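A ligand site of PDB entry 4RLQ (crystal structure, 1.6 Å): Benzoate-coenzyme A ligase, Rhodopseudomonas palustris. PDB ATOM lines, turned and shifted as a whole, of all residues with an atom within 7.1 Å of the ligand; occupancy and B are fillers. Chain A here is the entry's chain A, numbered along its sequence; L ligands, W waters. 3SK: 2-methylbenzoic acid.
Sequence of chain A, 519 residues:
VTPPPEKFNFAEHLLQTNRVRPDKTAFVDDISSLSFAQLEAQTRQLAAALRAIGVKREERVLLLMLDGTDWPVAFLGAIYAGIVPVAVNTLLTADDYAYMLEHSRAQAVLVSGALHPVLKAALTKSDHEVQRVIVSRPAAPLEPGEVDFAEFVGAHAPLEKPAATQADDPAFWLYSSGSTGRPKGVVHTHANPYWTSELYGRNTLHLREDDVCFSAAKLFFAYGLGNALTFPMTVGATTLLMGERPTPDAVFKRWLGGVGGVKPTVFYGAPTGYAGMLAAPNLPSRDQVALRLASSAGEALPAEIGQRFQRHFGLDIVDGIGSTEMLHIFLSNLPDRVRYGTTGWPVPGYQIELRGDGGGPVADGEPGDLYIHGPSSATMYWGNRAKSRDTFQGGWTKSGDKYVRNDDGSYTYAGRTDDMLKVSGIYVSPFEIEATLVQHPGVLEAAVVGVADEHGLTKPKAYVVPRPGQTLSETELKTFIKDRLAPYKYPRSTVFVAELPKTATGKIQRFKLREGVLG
N of Gly 322 lies within hydrogen-bond range of O8 of the ligand, at 2.9 Å. The backbone NH of Gly 298 sits close to an oxygen (O9) of the ligand.
The backbone carbonyl oxygen (O) of Ile 321 lies within hydrogen-bond range of the backbone NH (N) of Phe 330 (3.0 Å). The backbone carbonyl oxygen (O) of Tyr 223 is in hydrogen-bond range of a ring nitrogen (NE2) of His 328. The side-chain hydroxyl (OH) of Tyr 223 is in hydrogen-bond range of the backbone NH (N) of Ala 297, 3.5 Å away. The side-chain hydroxyl (OH) of Tyr 223 lies within hydrogen-bond range of the backbone NH (N) of Ser 296. The backbone carbonyl oxygen of Tyr 223 sits close to the side-chain amide oxygen of Asn 227 (2.9 Å). OG of Ser 323 is in hydrogen-bond range of N of Met 326. A ring nitrogen (NE2) of His 328 lies within hydrogen-bond range of the side-chain amide oxygen (OD1) of Asn 227 (3.0 Å). The backbone NH of Gly 320 is in hydrogen-bond range of the backbone carbonyl oxygen of Ser 296 (3.0 Å).
Residues that only touch the ligand: Ala 222 (3.6 Å), Tyr 223 (3.4 Å), Ala 297 (3.9 Å), Gly 320 (3.99 Å), Ile 321 (3.4 Å), Ser 323 (3.5 Å), Thr 324 (3.9 Å), Leu 327 (3.6 Å), His 328 (3.7 Å) and Ile 329 (3.9 Å). 12 residues have an atom within 4 Å of the ligand: Ala 222, Tyr 223, Ala 297, Gly 298, Gly 320, Ile 321, Gly 322, Ser 323, Thr 324, Leu 327, His 328 and Ile 329. The nearest printed residue that does not touch the ligand is Tyr 427 (5.1 Å).
Water W4 lies within hydrogen-bond range of O8 of the ligand (2.5 Å), O of Gly 320 (2.8 Å) and N of Gly 298 (2.9 Å). Water W2 bridges O9 of the ligand (2.9 Å) and NZ of Lys 422 (3.4 Å).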
ATOM      1  N   PHE A 221     -32.702  15.970  21.274  1.00  0.00           N
ATOM      2  CA  PHE A 221     -31.940  14.703  21.204  1.00  0.00           C
ATOM      3  C   PHE A 221     -32.944  13.555  21.458  1.00  0.00           C
ATOM      4  O   PHE A 221     -33.766  13.665  22.344  1.00  0.00           O
ATOM      5  CB  PHE A 221     -30.894  14.610  22.290  1.00  0.00           C
ATOM      6  CG  PHE A 221     -29.679  15.521  22.097  1.00  0.00           C
ATOM      7  CD1 PHE A 221     -28.797  15.266  21.031  1.00  0.00           C
ATOM      8  CD2 PHE A 221     -29.448  16.613  22.937  1.00  0.00           C
ATOM      9  CE1 PHE A 221     -27.645  16.048  20.853  1.00  0.00           C
ATOM     10  CE2 PHE A 221     -28.274  17.352  22.782  1.00  0.00           C
ATOM     11  CZ  PHE A 221     -27.382  17.077  21.757  1.00  0.00           C
ATOM     12  N   ALA A 222     -32.838  12.470  20.688  1.00  0.00           N
ATOM     13  CA  ALA A 222     -33.684  11.327  20.939  1.00  0.00           C
ATOM     14  C   ALA A 222     -33.600  10.975  22.444  1.00  0.00           C
ATOM     15  O   ALA A 222     -34.620  10.677  23.067  1.00  0.00           O
ATOM     16  CB  ALA A 222     -33.283  10.191  20.087  1.00  0.00           C
ATOM     17  N   TYR A 223     -32.399  10.904  22.988  1.00  0.00           N
ATOM     18  CA  TYR A 223     -32.198  10.591  24.435  1.00  0.00           C
ATOM     19  C   TYR A 223     -33.045  11.478  25.293  1.00  0.00           C
ATOM     20  O   TYR A 223     -33.859  10.986  26.118  1.00  0.00           O
ATOM     21  CB  TYR A 223     -30.710  10.645  24.741  1.00  0.00           C
ATOM     22  CG  TYR A 223     -30.316  10.280  26.163  1.00  0.00           C
ATOM     23  CD1 TYR A 223     -30.744   9.075  26.744  1.00  0.00           C
ATOM     24  CD2 TYR A 223     -29.468  11.088  26.884  1.00  0.00           C
ATOM     25  CE1 TYR A 223     -30.389   8.771  28.065  1.00  0.00           C
ATOM     26  CE2 TYR A 223     -29.067  10.725  28.160  1.00  0.00           C
ATOM     27  CZ  TYR A 223     -29.502   9.596  28.739  1.00  0.00           C
ATOM     28  OH  TYR A 223     -29.078   9.324  30.039  1.00  0.00           O
ATOM     29  N   GLY A 224     -32.931  12.802  25.101  1.00  0.00           N
ATOM     30  CA  GLY A 224     -33.668  13.733  25.912  1.00  0.00           C
ATOM     31  C   GLY A 224     -35.182  13.779  25.686  1.00  0.00           C
ATOM     32  O   GLY A 224     -35.969  13.950  26.633  1.00  0.00           O
ATOM     33  N   ASN A 227     -36.338  11.012  27.882  1.00  0.00           N
ATOM     34  CA  ASN A 227     -36.058  11.247  29.271  1.00  0.00           C
ATOM     35  C   ASN A 227     -36.982  12.289  29.885  1.00  0.00           C
ATOM     36  O   ASN A 227     -37.401  12.154  31.064  1.00  0.00           O
ATOM     37  CB  ASN A 227     -34.620  11.799  29.410  1.00  0.00           C
ATOM     38  CG  ASN A 227     -33.543  10.885  28.936  1.00  0.00           C
ATOM     39  OD1 ASN A 227     -33.704   9.684  28.732  1.00  0.00           O
ATOM     40  ND2 ASN A 227     -32.351  11.500  28.734  1.00  0.00           N
ATOM     41  N   SER A 296     -27.219   7.505  32.059  1.00  0.00           N
ATOM     42  CA  SER A 296     -26.178   7.992  31.205  1.00  0.00           C
ATOM     43  C   SER A 296     -26.231   7.459  29.798  1.00  0.00           C
ATOM     44  O   SER A 296     -26.473   6.271  29.596  1.00  0.00           O
ATOM     45  CB  SER A 296     -24.817   7.652  31.846  1.00  0.00           C
ATOM     46  OG  SER A 296     -23.739   8.232  31.135  1.00  0.00           O
ATOM     47  N   ALA A 297     -25.987   8.344  28.824  1.00  0.00           N
ATOM     48  CA  ALA A 297     -25.787   7.955  27.450  1.00  0.00           C
ATOM     49  C   ALA A 297     -25.071   9.032  26.694  1.00  0.00           C
ATOM     50  O   ALA A 297     -25.073  10.170  27.123  1.00  0.00           O
ATOM     51  CB  ALA A 297     -27.125   7.714  26.807  1.00  0.00           C
ATOM     52  N   GLY A 298     -24.590   8.659  25.512  1.00  0.00           N
ATOM     53  CA  GLY A 298     -24.027   9.618  24.586  1.00  0.00           C
ATOM     54  C   GLY A 298     -22.550   9.304  24.287  1.00  0.00           C
ATOM     55  O   GLY A 298     -22.012   9.745  23.279  1.00  0.00           O
ATOM     56  N   GLU A 299     -21.928   8.542  25.137  1.00  0.00           N
ATOM     57  CA  GLU A 299     -20.559   8.043  24.985  1.00  0.00           C
ATOM     58  C   GLU A 299     -20.438   6.942  26.068  1.00  0.00           C
ATOM     59  O   GLU A 299     -21.284   6.872  27.006  1.00  0.00           O
ATOM     60  CB  GLU A 299     -19.538   9.160  25.191  1.00  0.00           C
ATOM     61  CG  GLU A 299     -19.639   9.869  26.518  1.00  0.00           C
ATOM     62  CD  GLU A 299     -18.828  11.169  26.663  1.00  0.00           C
ATOM     63  OE1 GLU A 299     -17.710  11.286  26.099  1.00  0.00           O
ATOM     64  OE2 GLU A 299     -19.332  12.072  27.347  1.00  0.00           O
ATOM     65  N   ASP A 319     -25.666   3.215  32.588  1.00  0.00           N
ATOM     66  CA  ASP A 319     -25.186   3.542  31.216  1.00  0.00           C
ATOM     67  C   ASP A 319     -25.934   2.649  30.241  1.00  0.00           C
ATOM     68  O   ASP A 319     -25.943   1.417  30.372  1.00  0.00           O
ATOM     69  CB  ASP A 319     -23.665   3.272  31.201  1.00  0.00           C
ATOM     70  CG  ASP A 319     -23.019   3.226  29.839  1.00  0.00           C
ATOM     71  OD1 ASP A 319     -23.533   3.708  28.803  1.00  0.00           O
ATOM     72  OD2 ASP A 319     -21.800   2.818  29.823  1.00  0.00           O
ATOM     73  N   GLY A 320     -26.545   3.267  29.220  1.00  0.00           N
ATOM     74  CA  GLY A 320     -27.176   2.480  28.148  1.00  0.00           C
ATOM     75  C   GLY A 320     -26.838   3.145  26.804  1.00  0.00           C
ATOM     76  O   GLY A 320     -26.345   4.270  26.756  1.00  0.00           O
ATOM     77  N   ILE A 321     -27.146   2.429  25.723  1.00  0.00           N
ATOM     78  CA  ILE A 321     -26.935   2.917  24.363  1.00  0.00           C
ATOM     79  C   ILE A 321     -28.211   2.809  23.582  1.00  0.00           C
ATOM     80  O   ILE A 321     -28.859   1.783  23.620  1.00  0.00           O
ATOM     81  CB  ILE A 321     -25.763   2.222  23.651  1.00  0.00           C
ATOM     82  CG1 ILE A 321     -25.450   2.979  22.339  1.00  0.00           C
ATOM     83  CG2 ILE A 321     -25.925   0.700  23.481  1.00  0.00           C
ATOM     84  CD1 ILE A 321     -24.125   2.567  21.730  1.00  0.00           C
ATOM     85  N   GLY A 322     -28.492   3.893  22.870  1.00  0.00           N
ATOM     86  CA  GLY A 322     -29.515   3.925  21.869  1.00  0.00           C
ATOM     87  C   GLY A 322     -28.969   4.459  20.562  1.00  0.00           C
ATOM     88  O   GLY A 322     -27.783   4.571  20.325  1.00  0.00           O
ATOM     89  N   SER A 323     -29.909   4.779  19.666  1.00  0.00           N
ATOM     90  CA  SER A 323     -29.608   5.491  18.456  1.00  0.00           C
ATOM     91  C   SER A 323     -30.771   6.322  18.057  1.00  0.00           C
ATOM     92  O   SER A 323     -31.935   6.072  18.447  1.00  0.00           O
ATOM     93  CB  SER A 323     -29.289   4.546  17.305  1.00  0.00           C
ATOM     94  OG  SER A 323     -30.429   3.776  16.866  1.00  0.00           O
ATOM     95  N   THR A 324     -30.484   7.358  17.230  1.00  0.00           N
ATOM     96  CA  THR A 324     -31.579   8.161  16.717  1.00  0.00           C
ATOM     97  C   THR A 324     -32.615   7.327  15.956  1.00  0.00           C
ATOM     98  O   THR A 324     -33.833   7.447  16.156  1.00  0.00           O
ATOM     99  CB  THR A 324     -31.022   9.312  15.848  1.00  0.00           C
ATOM    100  OG1 THR A 324     -30.066  10.050  16.644  1.00  0.00           O
ATOM    101  CG2 THR A 324     -32.177  10.230  15.432  1.00  0.00           C
ATOM    102  N   GLU A 325     -32.099   6.386  15.191  1.00  0.00           N
ATOM    103  CA  GLU A 325     -32.957   5.473  14.399  1.00  0.00           C
ATOM    104  C   GLU A 325     -33.821   4.512  15.246  1.00  0.00           C
ATOM    105  O   GLU A 325     -34.917   4.123  14.849  1.00  0.00           O
ATOM    106  CB  GLU A 325     -32.109   4.727  13.408  1.00  0.00           C
ATOM    107  CG  GLU A 325     -31.421   5.625  12.362  1.00  0.00           C
ATOM    108  CD  GLU A 325     -30.073   6.181  12.779  1.00  0.00           C
ATOM    109  OE1 GLU A 325     -29.669   6.107  13.986  1.00  0.00           O
ATOM    110  OE2 GLU A 325     -29.446   6.831  11.856  1.00  0.00           O
ATOM    111  N   MET A 326     -33.340   4.068  16.413  1.00  0.00           N
ATOM    112  CA  MET A 326     -34.089   3.236  17.308  1.00  0.00           C
ATOM    113  C   MET A 326     -34.869   3.996  18.339  1.00  0.00           C
ATOM    114  O   MET A 326     -35.616   3.366  19.117  1.00  0.00           O
ATOM    115  CB  MET A 326     -33.213   2.211  17.983  1.00  0.00           C
ATOM    116  CG  MET A 326     -32.620   1.195  17.087  1.00  0.00           C
ATOM    117  SD  MET A 326     -33.791   0.270  16.048  1.00  0.00           S
ATOM    118  CE  MET A 326     -34.881  -0.507  17.251  1.00  0.00           C
ATOM    119  N   LEU A 327     -34.736   5.337  18.297  1.00  0.00           N
ATOM    120  CA  LEU A 327     -35.422   6.279  19.141  1.00  0.00           C
ATOM    121  C   LEU A 327     -34.964   6.350  20.600  1.00  0.00           C
ATOM    122  O   LEU A 327     -34.887   7.447  21.153  1.00  0.00           O
ATOM    123  CB  LEU A 327     -36.920   6.101  19.052  1.00  0.00           C
ATOM    124  CG  LEU A 327     -37.761   7.263  19.666  1.00  0.00           C
ATOM    125  CD1 LEU A 327     -37.426   8.718  19.205  1.00  0.00           C
ATOM    126  CD2 LEU A 327     -39.237   7.024  19.512  1.00  0.00           C
ATOM    127  N   HIS A 328     -34.728   5.210  21.217  1.00  0.00           N
ATOM    128  CA  HIS A 328     -34.119   5.248  22.609  1.00  0.00           C
ATOM    129  C   HIS A 328     -33.266   4.017  22.870  1.00  0.00           C
ATOM    130  O   HIS A 328     -32.859   3.336  21.952  1.00  0.00           O
ATOM    131  CB  HIS A 328     -35.210   5.580  23.671  1.00  0.00           C
ATOM    132  CG  HIS A 328     -34.668   6.396  24.828  1.00  0.00           C
ATOM    133  ND1 HIS A 328     -34.012   5.826  25.897  1.00  0.00           N
ATOM    134  CD2 HIS A 328     -34.741   7.731  25.102  1.00  0.00           C
ATOM    135  CE1 HIS A 328     -33.669   6.773  26.770  1.00  0.00           C
ATOM    136  NE2 HIS A 328     -34.107   7.930  26.321  1.00  0.00           N
ATOM    137  N   ILE A 329     -33.006   3.704  24.132  1.00  0.00           N
ATOM    138  CA  ILE A 329     -31.965   2.778  24.506  1.00  0.00           C
ATOM    139  C   ILE A 329     -32.462   1.334  24.314  1.00  0.00           C
ATOM    140  O   ILE A 329     -33.583   0.991  24.735  1.00  0.00           O
ATOM    141  CB  ILE A 329     -31.545   3.048  25.992  1.00  0.00           C
ATOM    142  CG1 ILE A 329     -30.681   4.348  26.018  1.00  0.00           C
ATOM    143  CG2 ILE A 329     -30.776   1.879  26.535  1.00  0.00           C
ATOM    144  CD1 ILE A 329     -30.392   4.865  27.406  1.00  0.00           C
ATOM    145  N   PHE A 330     -31.630   0.515  23.730  1.00  0.00           N
ATOM    146  CA  PHE A 330     -31.927  -0.882  23.488  1.00  0.00           C
ATOM    147  C   PHE A 330     -30.944  -1.848  24.144  1.00  0.00           C
ATOM    148  O   PHE A 330     -31.175  -3.063  24.082  1.00  0.00           O
ATOM    149  CB  PHE A 330     -32.004  -1.110  21.965  1.00  0.00           C
ATOM    150  CG  PHE A 330     -30.837  -0.552  21.218  1.00  0.00           C
ATOM    151  CD1 PHE A 330     -29.553  -1.094  21.360  1.00  0.00           C
ATOM    152  CD2 PHE A 330     -30.976   0.567  20.421  1.00  0.00           C
ATOM    153  CE1 PHE A 330     -28.469  -0.525  20.692  1.00  0.00           C
ATOM    154  CE2 PHE A 330     -29.894   1.116  19.744  1.00  0.00           C
ATOM    155  CZ  PHE A 330     -28.642   0.593  19.894  1.00  0.00           C
ATOM    156  N   ASP A 401     -22.162   1.067  15.624  1.00  0.00           N
ATOM    157  CA  ASP A 401     -21.237   0.753  16.699  1.00  0.00           C
ATOM    158  C   ASP A 401     -20.690  -0.682  16.474  1.00  0.00           C
ATOM    159  O   ASP A 401     -21.362  -1.511  15.825  1.00  0.00           O
ATOM    160  CB  ASP A 401     -21.950   0.734  18.045  1.00  0.00           C
ATOM    161  CG  ASP A 401     -22.659   2.051  18.348  1.00  0.00           C
ATOM    162  OD1 ASP A 401     -21.911   2.999  18.583  1.00  0.00           O
ATOM    163  OD2 ASP A 401     -23.917   2.130  18.335  1.00  0.00           O
ATOM    164  N   LYS A 422     -17.707  10.234  19.378  1.00  0.00           N
ATOM    165  CA  LYS A 422     -18.716  10.660  20.382  1.00  0.00           C
ATOM    166  C   LYS A 422     -17.956  11.457  21.434  1.00  0.00           C
ATOM    167  O   LYS A 422     -17.156  10.856  22.196  1.00  0.00           O
ATOM    168  CB  LYS A 422     -19.358   9.431  21.030  1.00  0.00           C
ATOM    169  CG  LYS A 422     -19.935   8.419  20.039  1.00  0.00           C
ATOM    170  CD  LYS A 422     -20.780   7.332  20.736  1.00  0.00           C
ATOM    171  CE  LYS A 422     -20.991   6.154  19.798  1.00  0.00           C
ATOM    172  NZ  LYS A 422     -21.920   5.105  20.335  1.00  0.00           N
ATOM    173  N   GLY A 425     -20.647  13.581  24.752  1.00  0.00           N
ATOM    174  CA  GLY A 425     -21.965  13.038  24.590  1.00  0.00           C
ATOM    175  C   GLY A 425     -22.641  13.289  23.263  1.00  0.00           C
ATOM    176  O   GLY A 425     -23.792  12.857  23.091  1.00  0.00           O
ATOM    177  N   TYR A 427     -22.371  13.358  18.706  1.00  0.00           N
ATOM    178  CA  TYR A 427     -21.673  12.802  17.518  1.00  0.00           C
ATOM    179  C   TYR A 427     -21.004  13.971  16.842  1.00  0.00           C
ATOM    180  O   TYR A 427     -21.643  15.030  16.649  1.00  0.00           O
ATOM    181  CB  TYR A 427     -22.619  12.153  16.548  1.00  0.00           C
ATOM    182  CG  TYR A 427     -22.956  10.729  16.793  1.00  0.00           C
ATOM    183  CD1 TYR A 427     -23.111  10.239  18.079  1.00  0.00           C
ATOM    184  CD2 TYR A 427     -23.225   9.866  15.731  1.00  0.00           C
ATOM    185  CE1 TYR A 427     -23.463   8.902  18.311  1.00  0.00           C
ATOM    186  CE2 TYR A 427     -23.586   8.539  15.952  1.00  0.00           C
ATOM    187  CZ  TYR A 427     -23.703   8.063  17.246  1.00  0.00           C
ATOM    188  OH  TYR A 427     -24.047   6.740  17.475  1.00  0.00           O
HETATM  189  O8  3SK L   1     -26.801   6.164  23.270  1.00  0.00           O
HETATM  190  C1  3SK L   1     -27.207   7.284  22.873  1.00  0.00           C
HETATM  191  O9  3SK L   1     -26.503   8.332  22.795  1.00  0.00           O
HETATM  192  C2  3SK L   1     -28.684   7.431  22.578  1.00  0.00           C
HETATM  193  C3  3SK L   1     -29.628   7.126  23.542  1.00  0.00           C
HETATM  194  C4  3SK L   1     -30.980   7.318  23.296  1.00  0.00           C
HETATM  195  C5  3SK L   1     -31.414   7.742  22.034  1.00  0.00           C
HETATM  196  C6  3SK L   1     -30.459   8.086  21.101  1.00  0.00           C
HETATM  197  C7  3SK L   1     -29.079   7.930  21.338  1.00  0.00           C
HETATM  198  C10 3SK L   1     -28.120   8.306  20.227  1.00  0.00           C
HETATM  199  O   HOH W   1     -29.937  11.426  21.487  1.00  0.00           O
HETATM  200  O   HOH W   2     -24.232   7.396  21.279  1.00  0.00           O
HETATM  201  O   HOH W   3     -27.416  10.765  22.676  1.00  0.00           O
HETATM  202  O   HOH W   4     -24.858   5.793  24.868  1.00  0.00           O
